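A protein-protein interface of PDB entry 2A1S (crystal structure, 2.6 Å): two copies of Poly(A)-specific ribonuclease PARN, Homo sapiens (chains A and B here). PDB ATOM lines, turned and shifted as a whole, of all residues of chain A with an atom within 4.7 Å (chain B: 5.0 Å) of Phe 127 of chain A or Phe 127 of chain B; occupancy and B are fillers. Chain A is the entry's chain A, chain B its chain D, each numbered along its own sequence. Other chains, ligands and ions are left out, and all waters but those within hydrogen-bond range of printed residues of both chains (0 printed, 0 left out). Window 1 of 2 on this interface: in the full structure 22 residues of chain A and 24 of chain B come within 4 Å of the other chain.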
ATOM      1  N   PHE A  67     -12.790  -4.460 -27.297  1.00  0.00           N
ATOM      2  CA  PHE A  67     -13.612  -3.891 -26.235  1.00  0.00           C
ATOM      3  C   PHE A  67     -13.470  -2.396 -26.001  1.00  0.00           C
ATOM      4  O   PHE A  67     -14.144  -1.868 -25.141  1.00  0.00           O
ATOM      5  CB  PHE A  67     -13.548  -4.667 -24.909  1.00  0.00           C
ATOM      6  CG  PHE A  67     -12.170  -4.944 -24.393  1.00  0.00           C
ATOM      7  CD1 PHE A  67     -11.091  -4.147 -24.721  1.00  0.00           C
ATOM      8  CD2 PHE A  67     -11.968  -6.014 -23.531  1.00  0.00           C
ATOM      9  CE1 PHE A  67      -9.859  -4.431 -24.227  1.00  0.00           C
ATOM     10  CE2 PHE A  67     -10.726  -6.288 -23.032  1.00  0.00           C
ATOM     11  CZ  PHE A  67      -9.678  -5.511 -23.379  1.00  0.00           C
ATOM     12  N   PHE A  93     -19.128  -4.411 -24.647  1.00  0.00           N
ATOM     13  CA  PHE A  93     -19.267  -5.790 -24.219  1.00  0.00           C
ATOM     14  C   PHE A  93     -20.587  -6.391 -24.750  1.00  0.00           C
ATOM     15  O   PHE A  93     -21.613  -5.712 -24.783  1.00  0.00           O
ATOM     16  CB  PHE A  93     -19.260  -5.836 -22.693  1.00  0.00           C
ATOM     17  CG  PHE A  93     -19.006  -7.201 -22.122  1.00  0.00           C
ATOM     18  CD1 PHE A  93     -17.822  -7.865 -22.379  1.00  0.00           C
ATOM     19  CD2 PHE A  93     -19.932  -7.803 -21.305  1.00  0.00           C
ATOM     20  CE1 PHE A  93     -17.585  -9.132 -21.848  1.00  0.00           C
ATOM     21  CE2 PHE A  93     -19.700  -9.065 -20.776  1.00  0.00           C
ATOM     22  CZ  PHE A  93     -18.528  -9.731 -21.057  1.00  0.00           C
ATOM     23  N   PHE A 106     -15.233 -15.465 -25.157  1.00  0.00           N
ATOM     24  CA  PHE A 106     -14.108 -14.849 -25.843  1.00  0.00           C
ATOM     25  C   PHE A 106     -12.832 -15.196 -25.088  1.00  0.00           C
ATOM     26  O   PHE A 106     -12.870 -15.715 -23.981  1.00  0.00           O
ATOM     27  CB  PHE A 106     -14.299 -13.328 -25.964  1.00  0.00           C
ATOM     28  CG  PHE A 106     -14.494 -12.657 -24.660  1.00  0.00           C
ATOM     29  CD1 PHE A 106     -13.416 -12.145 -23.960  1.00  0.00           C
ATOM     30  CD2 PHE A 106     -15.746 -12.603 -24.086  1.00  0.00           C
ATOM     31  CE1 PHE A 106     -13.590 -11.553 -22.705  1.00  0.00           C
ATOM     32  CE2 PHE A 106     -15.933 -12.014 -22.837  1.00  0.00           C
ATOM     33  CZ  PHE A 106     -14.846 -11.481 -22.152  1.00  0.00           C
ATOM     34  N   ILE A 113      -3.597  -7.889 -21.740  1.00  0.00           N
ATOM     35  CA  ILE A 113      -4.326  -7.396 -20.587  1.00  0.00           C
ATOM     36  C   ILE A 113      -3.418  -6.655 -19.614  1.00  0.00           C
ATOM     37  O   ILE A 113      -3.809  -5.637 -19.034  1.00  0.00           O
ATOM     38  CB  ILE A 113      -5.061  -8.558 -19.906  1.00  0.00           C
ATOM     39  CG1 ILE A 113      -6.320  -8.869 -20.725  1.00  0.00           C
ATOM     40  CG2 ILE A 113      -5.379  -8.221 -18.438  1.00  0.00           C
ATOM     41  CD1 ILE A 113      -7.335  -9.693 -20.011  1.00  0.00           C
ATOM     42  N   ALA A 117      -3.520  -2.637 -18.493  1.00  0.00           N
ATOM     43  CA  ALA A 117      -3.481  -2.332 -17.069  1.00  0.00           C
ATOM     44  C   ALA A 117      -2.412  -1.276 -16.736  1.00  0.00           C
ATOM     45  O   ALA A 117      -2.621  -0.389 -15.911  1.00  0.00           O
ATOM     46  CB  ALA A 117      -3.217  -3.602 -16.299  1.00  0.00           C
ATOM     47  N   PHE A 123     -11.097  -1.683 -16.787  1.00  0.00           N
ATOM     48  CA  PHE A 123     -11.769  -2.934 -17.186  1.00  0.00           C
ATOM     49  C   PHE A 123     -13.177  -3.026 -16.669  1.00  0.00           C
ATOM     50  O   PHE A 123     -13.948  -3.857 -17.125  1.00  0.00           O
ATOM     51  CB  PHE A 123     -10.964  -4.165 -16.723  1.00  0.00           C
ATOM     52  CG  PHE A 123      -9.640  -4.280 -17.400  1.00  0.00           C
ATOM     53  CD1 PHE A 123      -8.487  -3.817 -16.775  1.00  0.00           C
ATOM     54  CD2 PHE A 123      -9.558  -4.757 -18.692  1.00  0.00           C
ATOM     55  CE1 PHE A 123      -7.263  -3.881 -17.415  1.00  0.00           C
ATOM     56  CE2 PHE A 123      -8.349  -4.836 -19.339  1.00  0.00           C
ATOM     57  CZ  PHE A 123      -7.179  -4.394 -18.700  1.00  0.00           C
ATOM     58  N   ASN A 124     -13.506  -2.176 -15.701  1.00  0.00           N
ATOM     59  CA  ASN A 124     -14.880  -2.073 -15.232  1.00  0.00           C
ATOM     60  C   ASN A 124     -15.771  -1.340 -16.232  1.00  0.00           C
ATOM     61  O   ASN A 124     -16.974  -1.570 -16.261  1.00  0.00           O
ATOM     62  CB  ASN A 124     -14.923  -1.408 -13.869  1.00  0.00           C
ATOM     63  CG  ASN A 124     -14.590  -2.360 -12.749  1.00  0.00           C
ATOM     64  OD1 ASN A 124     -14.885  -3.558 -12.820  1.00  0.00           O
ATOM     65  ND2 ASN A 124     -13.988  -1.827 -11.682  1.00  0.00           N
ATOM     66  N   LYS A 125     -15.192  -0.467 -17.053  1.00  0.00           N
ATOM     67  CA  LYS A 125     -15.963   0.190 -18.112  1.00  0.00           C
ATOM     68  C   LYS A 125     -16.317  -0.801 -19.229  1.00  0.00           C
ATOM     69  O   LYS A 125     -17.372  -0.721 -19.832  1.00  0.00           O
ATOM     70  CB  LYS A 125     -15.253   1.450 -18.650  1.00  0.00           C
ATOM     71  CG  LYS A 125     -15.485   2.701 -17.773  1.00  0.00           C
ATOM     72  CD  LYS A 125     -14.581   3.853 -18.123  1.00  0.00           C
ATOM     73  CE  LYS A 125     -14.938   5.063 -17.277  1.00  0.00           C
ATOM     74  NZ  LYS A 125     -14.190   6.285 -17.655  1.00  0.00           N
ATOM     75  N   VAL A 126     -15.462  -1.781 -19.460  1.00  0.00           N
ATOM     76  CA  VAL A 126     -15.807  -2.874 -20.359  1.00  0.00           C
ATOM     77  C   VAL A 126     -16.779  -3.884 -19.724  1.00  0.00           C
ATOM     78  O   VAL A 126     -17.872  -4.122 -20.241  1.00  0.00           O
ATOM     79  CB  VAL A 126     -14.553  -3.585 -20.840  1.00  0.00           C
ATOM     80  CG1 VAL A 126     -14.925  -4.758 -21.732  1.00  0.00           C
ATOM     81  CG2 VAL A 126     -13.647  -2.590 -21.591  1.00  0.00           C
ATOM     82  N   PHE A 127     -16.402  -4.455 -18.592  1.00  0.00           N
ATOM     83  CA  PHE A 127     -17.127  -5.603 -18.043  1.00  0.00           C
ATOM     84  C   PHE A 127     -18.299  -5.291 -17.121  1.00  0.00           C
ATOM     85  O   PHE A 127     -19.119  -6.152 -16.847  1.00  0.00           O
ATOM     86  CB  PHE A 127     -16.143  -6.510 -17.318  1.00  0.00           C
ATOM     87  CG  PHE A 127     -15.040  -7.004 -18.185  1.00  0.00           C
ATOM     88  CD1 PHE A 127     -13.718  -6.961 -17.747  1.00  0.00           C
ATOM     89  CD2 PHE A 127     -15.308  -7.525 -19.432  1.00  0.00           C
ATOM     90  CE1 PHE A 127     -12.683  -7.428 -18.549  1.00  0.00           C
ATOM     91  CE2 PHE A 127     -14.274  -8.004 -20.239  1.00  0.00           C
ATOM     92  CZ  PHE A 127     -12.960  -7.956 -19.793  1.00  0.00           C
ATOM     93  N   ARG A 128     -18.382  -4.067 -16.644  1.00  0.00           N
ATOM     94  CA  ARG A 128     -19.397  -3.700 -15.661  1.00  0.00           C
ATOM     95  C   ARG A 128     -20.417  -2.712 -16.196  1.00  0.00           C
ATOM     96  O   ARG A 128     -21.445  -2.503 -15.557  1.00  0.00           O
ATOM     97  CB  ARG A 128     -18.721  -3.092 -14.432  1.00  0.00           C
ATOM     98  CG  ARG A 128     -18.632  -3.969 -13.207  1.00  0.00           C
ATOM     99  CD  ARG A 128     -19.113  -3.263 -11.962  1.00  0.00           C
ATOM    100  NE  ARG A 128     -18.202  -3.362 -10.816  1.00  0.00           N
ATOM    101  CZ  ARG A 128     -17.374  -2.414 -10.377  1.00  0.00           C
ATOM    102  NH1 ARG A 128     -17.254  -1.246 -10.983  1.00  0.00           N
ATOM    103  NH2 ARG A 128     -16.631  -2.652  -9.307  1.00  0.00           N
ATOM    104  N   ASN A 129     -20.127  -2.081 -17.336  1.00  0.00           N
ATOM    105  CA  ASN A 129     -20.992  -1.048 -17.917  1.00  0.00           C
ATOM    106  C   ASN A 129     -20.533  -0.758 -19.349  1.00  0.00           C
ATOM    107  O   ASN A 129     -20.299   0.360 -19.725  1.00  0.00           O
ATOM    108  CB  ASN A 129     -20.944   0.227 -17.053  1.00  0.00           C
ATOM    109  CG  ASN A 129     -22.102   1.150 -17.307  1.00  0.00           C
ATOM    110  OD1 ASN A 129     -23.066   1.189 -16.551  1.00  0.00           O
ATOM    111  ND2 ASN A 129     -22.009   1.915 -18.365  1.00  0.00           N
ATOM    112  N   PHE B  67     -10.291 -16.481 -10.617  1.00  0.00           N
ATOM    113  CA  PHE B  67      -9.674 -15.204 -10.382  1.00  0.00           C
ATOM    114  C   PHE B  67     -10.114 -14.529  -9.112  1.00  0.00           C
ATOM    115  O   PHE B  67      -9.715 -13.447  -8.853  1.00  0.00           O
ATOM    116  CB  PHE B  67      -9.704 -14.289 -11.612  1.00  0.00           C
ATOM    117  CG  PHE B  67     -11.080 -13.988 -12.209  1.00  0.00           C
ATOM    118  CD1 PHE B  67     -12.264 -14.220 -11.543  1.00  0.00           C
ATOM    119  CD2 PHE B  67     -11.149 -13.405 -13.473  1.00  0.00           C
ATOM    120  CE1 PHE B  67     -13.503 -13.901 -12.147  1.00  0.00           C
ATOM    121  CE2 PHE B  67     -12.372 -13.068 -14.055  1.00  0.00           C
ATOM    122  CZ  PHE B  67     -13.544 -13.317 -13.390  1.00  0.00           C
ATOM    123  N   PHE B  93      -4.188 -13.230 -10.847  1.00  0.00           N
ATOM    124  CA  PHE B  93      -4.058 -13.084 -12.274  1.00  0.00           C
ATOM    125  C   PHE B  93      -2.691 -13.556 -12.716  1.00  0.00           C
ATOM    126  O   PHE B  93      -1.715 -13.162 -12.104  1.00  0.00           O
ATOM    127  CB  PHE B  93      -4.202 -11.639 -12.640  1.00  0.00           C
ATOM    128  CG  PHE B  93      -4.289 -11.434 -14.075  1.00  0.00           C
ATOM    129  CD1 PHE B  93      -5.456 -11.751 -14.744  1.00  0.00           C
ATOM    130  CD2 PHE B  93      -3.212 -10.960 -14.785  1.00  0.00           C
ATOM    131  CE1 PHE B  93      -5.543 -11.578 -16.096  1.00  0.00           C
ATOM    132  CE2 PHE B  93      -3.299 -10.764 -16.133  1.00  0.00           C
ATOM    133  CZ  PHE B  93      -4.459 -11.088 -16.796  1.00  0.00           C
ATOM    134  N   PHE B 106      -6.664 -17.198 -21.547  1.00  0.00           N
ATOM    135  CA  PHE B 106      -7.804 -17.850 -20.897  1.00  0.00           C
ATOM    136  C   PHE B 106      -9.109 -17.448 -21.575  1.00  0.00           C
ATOM    137  O   PHE B 106      -9.111 -16.573 -22.425  1.00  0.00           O
ATOM    138  CB  PHE B 106      -7.833 -17.523 -19.409  1.00  0.00           C
ATOM    139  CG  PHE B 106      -7.906 -16.055 -19.114  1.00  0.00           C
ATOM    140  CD1 PHE B 106      -9.089 -15.473 -18.678  1.00  0.00           C
ATOM    141  CD2 PHE B 106      -6.782 -15.255 -19.249  1.00  0.00           C
ATOM    142  CE1 PHE B 106      -9.155 -14.112 -18.406  1.00  0.00           C
ATOM    143  CE2 PHE B 106      -6.840 -13.906 -18.967  1.00  0.00           C
ATOM    144  CZ  PHE B 106      -8.031 -13.335 -18.551  1.00  0.00           C
ATOM    145  N   ILE B 113     -19.369 -13.072 -16.569  1.00  0.00           N
ATOM    146  CA  ILE B 113     -18.828 -11.732 -16.331  1.00  0.00           C
ATOM    147  C   ILE B 113     -19.975 -10.811 -15.970  1.00  0.00           C
ATOM    148  O   ILE B 113     -19.852  -9.973 -15.065  1.00  0.00           O
ATOM    149  CB  ILE B 113     -18.031 -11.201 -17.540  1.00  0.00           C
ATOM    150  CG1 ILE B 113     -16.573 -11.605 -17.397  1.00  0.00           C
ATOM    151  CG2 ILE B 113     -18.049  -9.688 -17.602  1.00  0.00           C
ATOM    152  CD1 ILE B 113     -16.358 -13.032 -17.601  1.00  0.00           C
ATOM    153  N   ALA B 117     -20.572  -8.807 -12.583  1.00  0.00           N
ATOM    154  CA  ALA B 117     -20.676  -7.366 -12.777  1.00  0.00           C
ATOM    155  C   ALA B 117     -21.897  -6.871 -12.027  1.00  0.00           C
ATOM    156  O   ALA B 117     -21.881  -5.794 -11.418  1.00  0.00           O
ATOM    157  CB  ALA B 117     -20.775  -7.042 -14.242  1.00  0.00           C
ATOM    158  N   PHE B 123     -13.337  -5.806 -11.521  1.00  0.00           N
ATOM    159  CA  PHE B 123     -12.440  -6.469 -12.449  1.00  0.00           C
ATOM    160  C   PHE B 123     -11.089  -5.813 -12.478  1.00  0.00           C
ATOM    161  O   PHE B 123     -10.117  -6.460 -12.834  1.00  0.00           O
ATOM    162  CB  PHE B 123     -13.045  -6.517 -13.862  1.00  0.00           C
ATOM    163  CG  PHE B 123     -14.343  -7.261 -13.921  1.00  0.00           C
ATOM    164  CD1 PHE B 123     -15.528  -6.613 -13.694  1.00  0.00           C
ATOM    165  CD2 PHE B 123     -14.363  -8.615 -14.159  1.00  0.00           C
ATOM    166  CE1 PHE B 123     -16.700  -7.282 -13.719  1.00  0.00           C
ATOM    167  CE2 PHE B 123     -15.544  -9.305 -14.193  1.00  0.00           C
ATOM    168  CZ  PHE B 123     -16.714  -8.644 -13.966  1.00  0.00           C
ATOM    169  N   ASN B 124     -10.997  -4.532 -12.138  1.00  0.00           N
ATOM    170  CA  ASN B 124      -9.679  -3.921 -12.032  1.00  0.00           C
ATOM    171  C   ASN B 124      -8.841  -4.584 -10.940  1.00  0.00           C
ATOM    172  O   ASN B 124      -7.649  -4.666 -11.088  1.00  0.00           O
ATOM    173  CB  ASN B 124      -9.757  -2.429 -11.802  1.00  0.00           C
ATOM    174  CG  ASN B 124     -10.281  -1.680 -13.015  1.00  0.00           C
ATOM    175  OD1 ASN B 124      -9.863  -1.918 -14.156  1.00  0.00           O
ATOM    176  ND2 ASN B 124     -11.202  -0.758 -12.769  1.00  0.00           N
ATOM    177  N   LYS B 125      -9.463  -5.096  -9.877  1.00  0.00           N
ATOM    178  CA  LYS B 125      -8.740  -5.861  -8.851  1.00  0.00           C
ATOM    179  C   LYS B 125      -8.151  -7.192  -9.351  1.00  0.00           C
ATOM    180  O   LYS B 125      -7.217  -7.720  -8.768  1.00  0.00           O
ATOM    181  CB  LYS B 125      -9.622  -6.100  -7.619  1.00  0.00           C
ATOM    182  CG  LYS B 125      -9.810  -4.852  -6.752  1.00  0.00           C
ATOM    183  CD  LYS B 125     -10.587  -5.117  -5.467  1.00  0.00           C
ATOM    184  CE  LYS B 125     -10.897  -3.810  -4.722  1.00  0.00           C
ATOM    185  NZ  LYS B 125     -12.118  -3.904  -3.877  1.00  0.00           N
ATOM    186  N   VAL B 126      -8.674  -7.734 -10.435  1.00  0.00           N
ATOM    187  CA  VAL B 126      -8.046  -8.897 -11.036  1.00  0.00           C
ATOM    188  C   VAL B 126      -7.079  -8.475 -12.166  1.00  0.00           C
ATOM    189  O   VAL B 126      -5.877  -8.827 -12.166  1.00  0.00           O
ATOM    190  CB  VAL B 126      -9.120  -9.896 -11.553  1.00  0.00           C
ATOM    191  CG1 VAL B 126      -8.499 -10.979 -12.403  1.00  0.00           C
ATOM    192  CG2 VAL B 126      -9.870 -10.531 -10.394  1.00  0.00           C
ATOM    193  N   PHE B 127      -7.609  -7.730 -13.132  1.00  0.00           N
ATOM    194  CA  PHE B 127      -6.880  -7.457 -14.373  1.00  0.00           C
ATOM    195  C   PHE B 127      -5.845  -6.349 -14.268  1.00  0.00           C
ATOM    196  O   PHE B 127      -4.932  -6.269 -15.081  1.00  0.00           O
ATOM    197  CB  PHE B 127      -7.865  -7.116 -15.486  1.00  0.00           C
ATOM    198  CG  PHE B 127      -8.761  -8.251 -15.866  1.00  0.00           C
ATOM    199  CD1 PHE B 127     -10.099  -8.056 -16.055  1.00  0.00           C
ATOM    200  CD2 PHE B 127      -8.257  -9.521 -16.041  1.00  0.00           C
ATOM    201  CE1 PHE B 127     -10.919  -9.102 -16.398  1.00  0.00           C
ATOM    202  CE2 PHE B 127      -9.098 -10.563 -16.393  1.00  0.00           C
ATOM    203  CZ  PHE B 127     -10.423 -10.341 -16.574  1.00  0.00           C
ATOM    204  N   ARG B 128      -5.985  -5.486 -13.276  1.00  0.00           N
ATOM    205  CA  ARG B 128      -5.081  -4.367 -13.133  1.00  0.00           C
ATOM    206  C   ARG B 128      -4.110  -4.590 -11.984  1.00  0.00           C
ATOM    207  O   ARG B 128      -2.967  -4.102 -12.036  1.00  0.00           O
ATOM    208  CB  ARG B 128      -5.856  -3.051 -12.980  1.00  0.00           C
ATOM    209  CG  ARG B 128      -5.150  -1.891 -13.646  1.00  0.00           C
ATOM    210  CD  ARG B 128      -6.029  -0.779 -14.124  1.00  0.00           C
ATOM    211  NE  ARG B 128      -6.813  -0.180 -13.052  1.00  0.00           N
ATOM    212  CZ  ARG B 128      -7.564   0.905 -13.195  1.00  0.00           C
ATOM    213  NH1 ARG B 128      -7.658   1.518 -14.363  1.00  0.00           N
ATOM    214  NH2 ARG B 128      -8.233   1.384 -12.156  1.00  0.00           N
ATOM    215  N   ASN B 129      -4.540  -5.331 -10.967  1.00  0.00           N
ATOM    216  CA  ASN B 129      -3.719  -5.525  -9.783  1.00  0.00           C
ATOM    217  C   ASN B 129      -3.958  -6.853  -9.046  1.00  0.00           C
ATOM    218  O   ASN B 129      -4.239  -6.877  -7.855  1.00  0.00           O
ATOM    219  CB  ASN B 129      -3.900  -4.351  -8.828  1.00  0.00           C
ATOM    220  CG  ASN B 129      -2.733  -4.218  -7.866  1.00  0.00           C
ATOM    221  OD1 ASN B 129      -1.591  -4.213  -8.287  1.00  0.00           O
ATOM    222  ND2 ASN B 129      -3.016  -4.151  -6.580  1.00  0.00           N
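The backbone NH (N) of Phe 123 of chain B is in hydrogen-bond range of the side-chain amide oxygen (OD1) of Asn 124 of chain A. N of Phe 123 of chain A sits at hydrogen-bond distance from OD1 of Asn 124 of chain B, at 2.9 Å. The side-chain amide nitrogen (ND2) of Asn 124 of chain B lies close to the side-chain amide nitrogen (ND2) of Asn 124 of chain A.
The side-chain amide nitrogen (ND2) of Asn 124 of chain A sits close to the guanidinium group (NH1) of Arg 128 of chain A (3.4 Å). O of Asn 124 of chain B sits at hydrogen-bond distance from N of Asn 129 of chain B (3.2 Å). O of Asn 124 of chain A sits at hydrogen-bond distance from N of Asn 129 of chain A.
Among the printed residues, pairs that only touch across the chains: Phe 127 of chain A with Ala 117 of chain B (3.2 Å), Phe 127 of chain A with Phe 127 of chain B (3.2 Å), Ala 117 of chain A with Phe 127 of chain B (3.4 Å), Ile 113 of chain A with Phe 93 of chain B (3.4 Å), Phe 93 of chain A with Ile 113 of chain B (3.5 Å), Phe 123 of chain A with Phe 127 of chain B (3.6 Å), Phe 127 of chain A with Phe 123 of chain B (3.7 Å), Ala 117 of chain A with Arg 128 of chain B (3.7 Å), Phe 127 of chain A with Ile 113 of chain B (3.7 Å), Arg 128 of chain A with Ala 117 of chain B (3.8 Å), Arg 128 of chain A with Phe 123 of chain B (3.9 Å), Ile 113 of chain A with Phe 127 of chain B (3.9 Å) and Ile 113 of chain A with Phe 106 of chain B (3.98 Å).
Phe 127 of chain A touches four residues of chain B. Of chain A, only Ile 113, Ala 117, Phe 123 and Phe 127 come within 4 Å of Phe 127 of chain B. Of the printed residues of chain A, Phe 123 of chain B touches Asn 124, Phe 127 and Arg 128. Printed residues of chain B within 4 Å of Phe 123 of chain A: Asn 124 (2.9 Å) and Phe 127 (3.6 Å). Lys 125 of chain B touches none of the printed residues of chain A. The nearest printed residue of chain A that does not touch Ala 117 of chain B is Asn 129 of chain A (5.9 Å).
Of the 12 printed residues of chain B, 8 touch a printed residue of chain A. Along chain B the printed residues that touch a printed residue of chain A span positions 93 to 128. Of the 12 printed residues of chain A, 7 touch a printed residue of chain B. Printed residues of chain A that touch a printed residue of chain B: Phe 93, Ile 113, Ala 117, Phe 123, Asn 124, Phe 127 and Arg 128. Hydrophobic or aromatic side chains of chain A that line the printed part of chain B: Phe 93, Ile 113, Ala 117, Phe 123 and Phe 127. Among the printed residues, 16 pairs touch across the chains.
Ile 113 of chain A touches Phe 127 of chain B, and with the chains exchanged Phe 127 of chain A touches Ile 113 of chain B. Ala 117 of chain A touches Arg 128 of chain B, and with the chains exchanged Arg 128 of chain A touches Ala 117 of chain B. Phe 123 of chain A touches Asn 124 of chain B, and with the chains exchanged Asn 124 of chain A touches Phe 123 of chain B. Arg 128 of chain A touches Phe 123 of chain B, but with the chains exchanged Phe 123 of chain A does not touch Arg 128 of chain B (4.6 Å).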
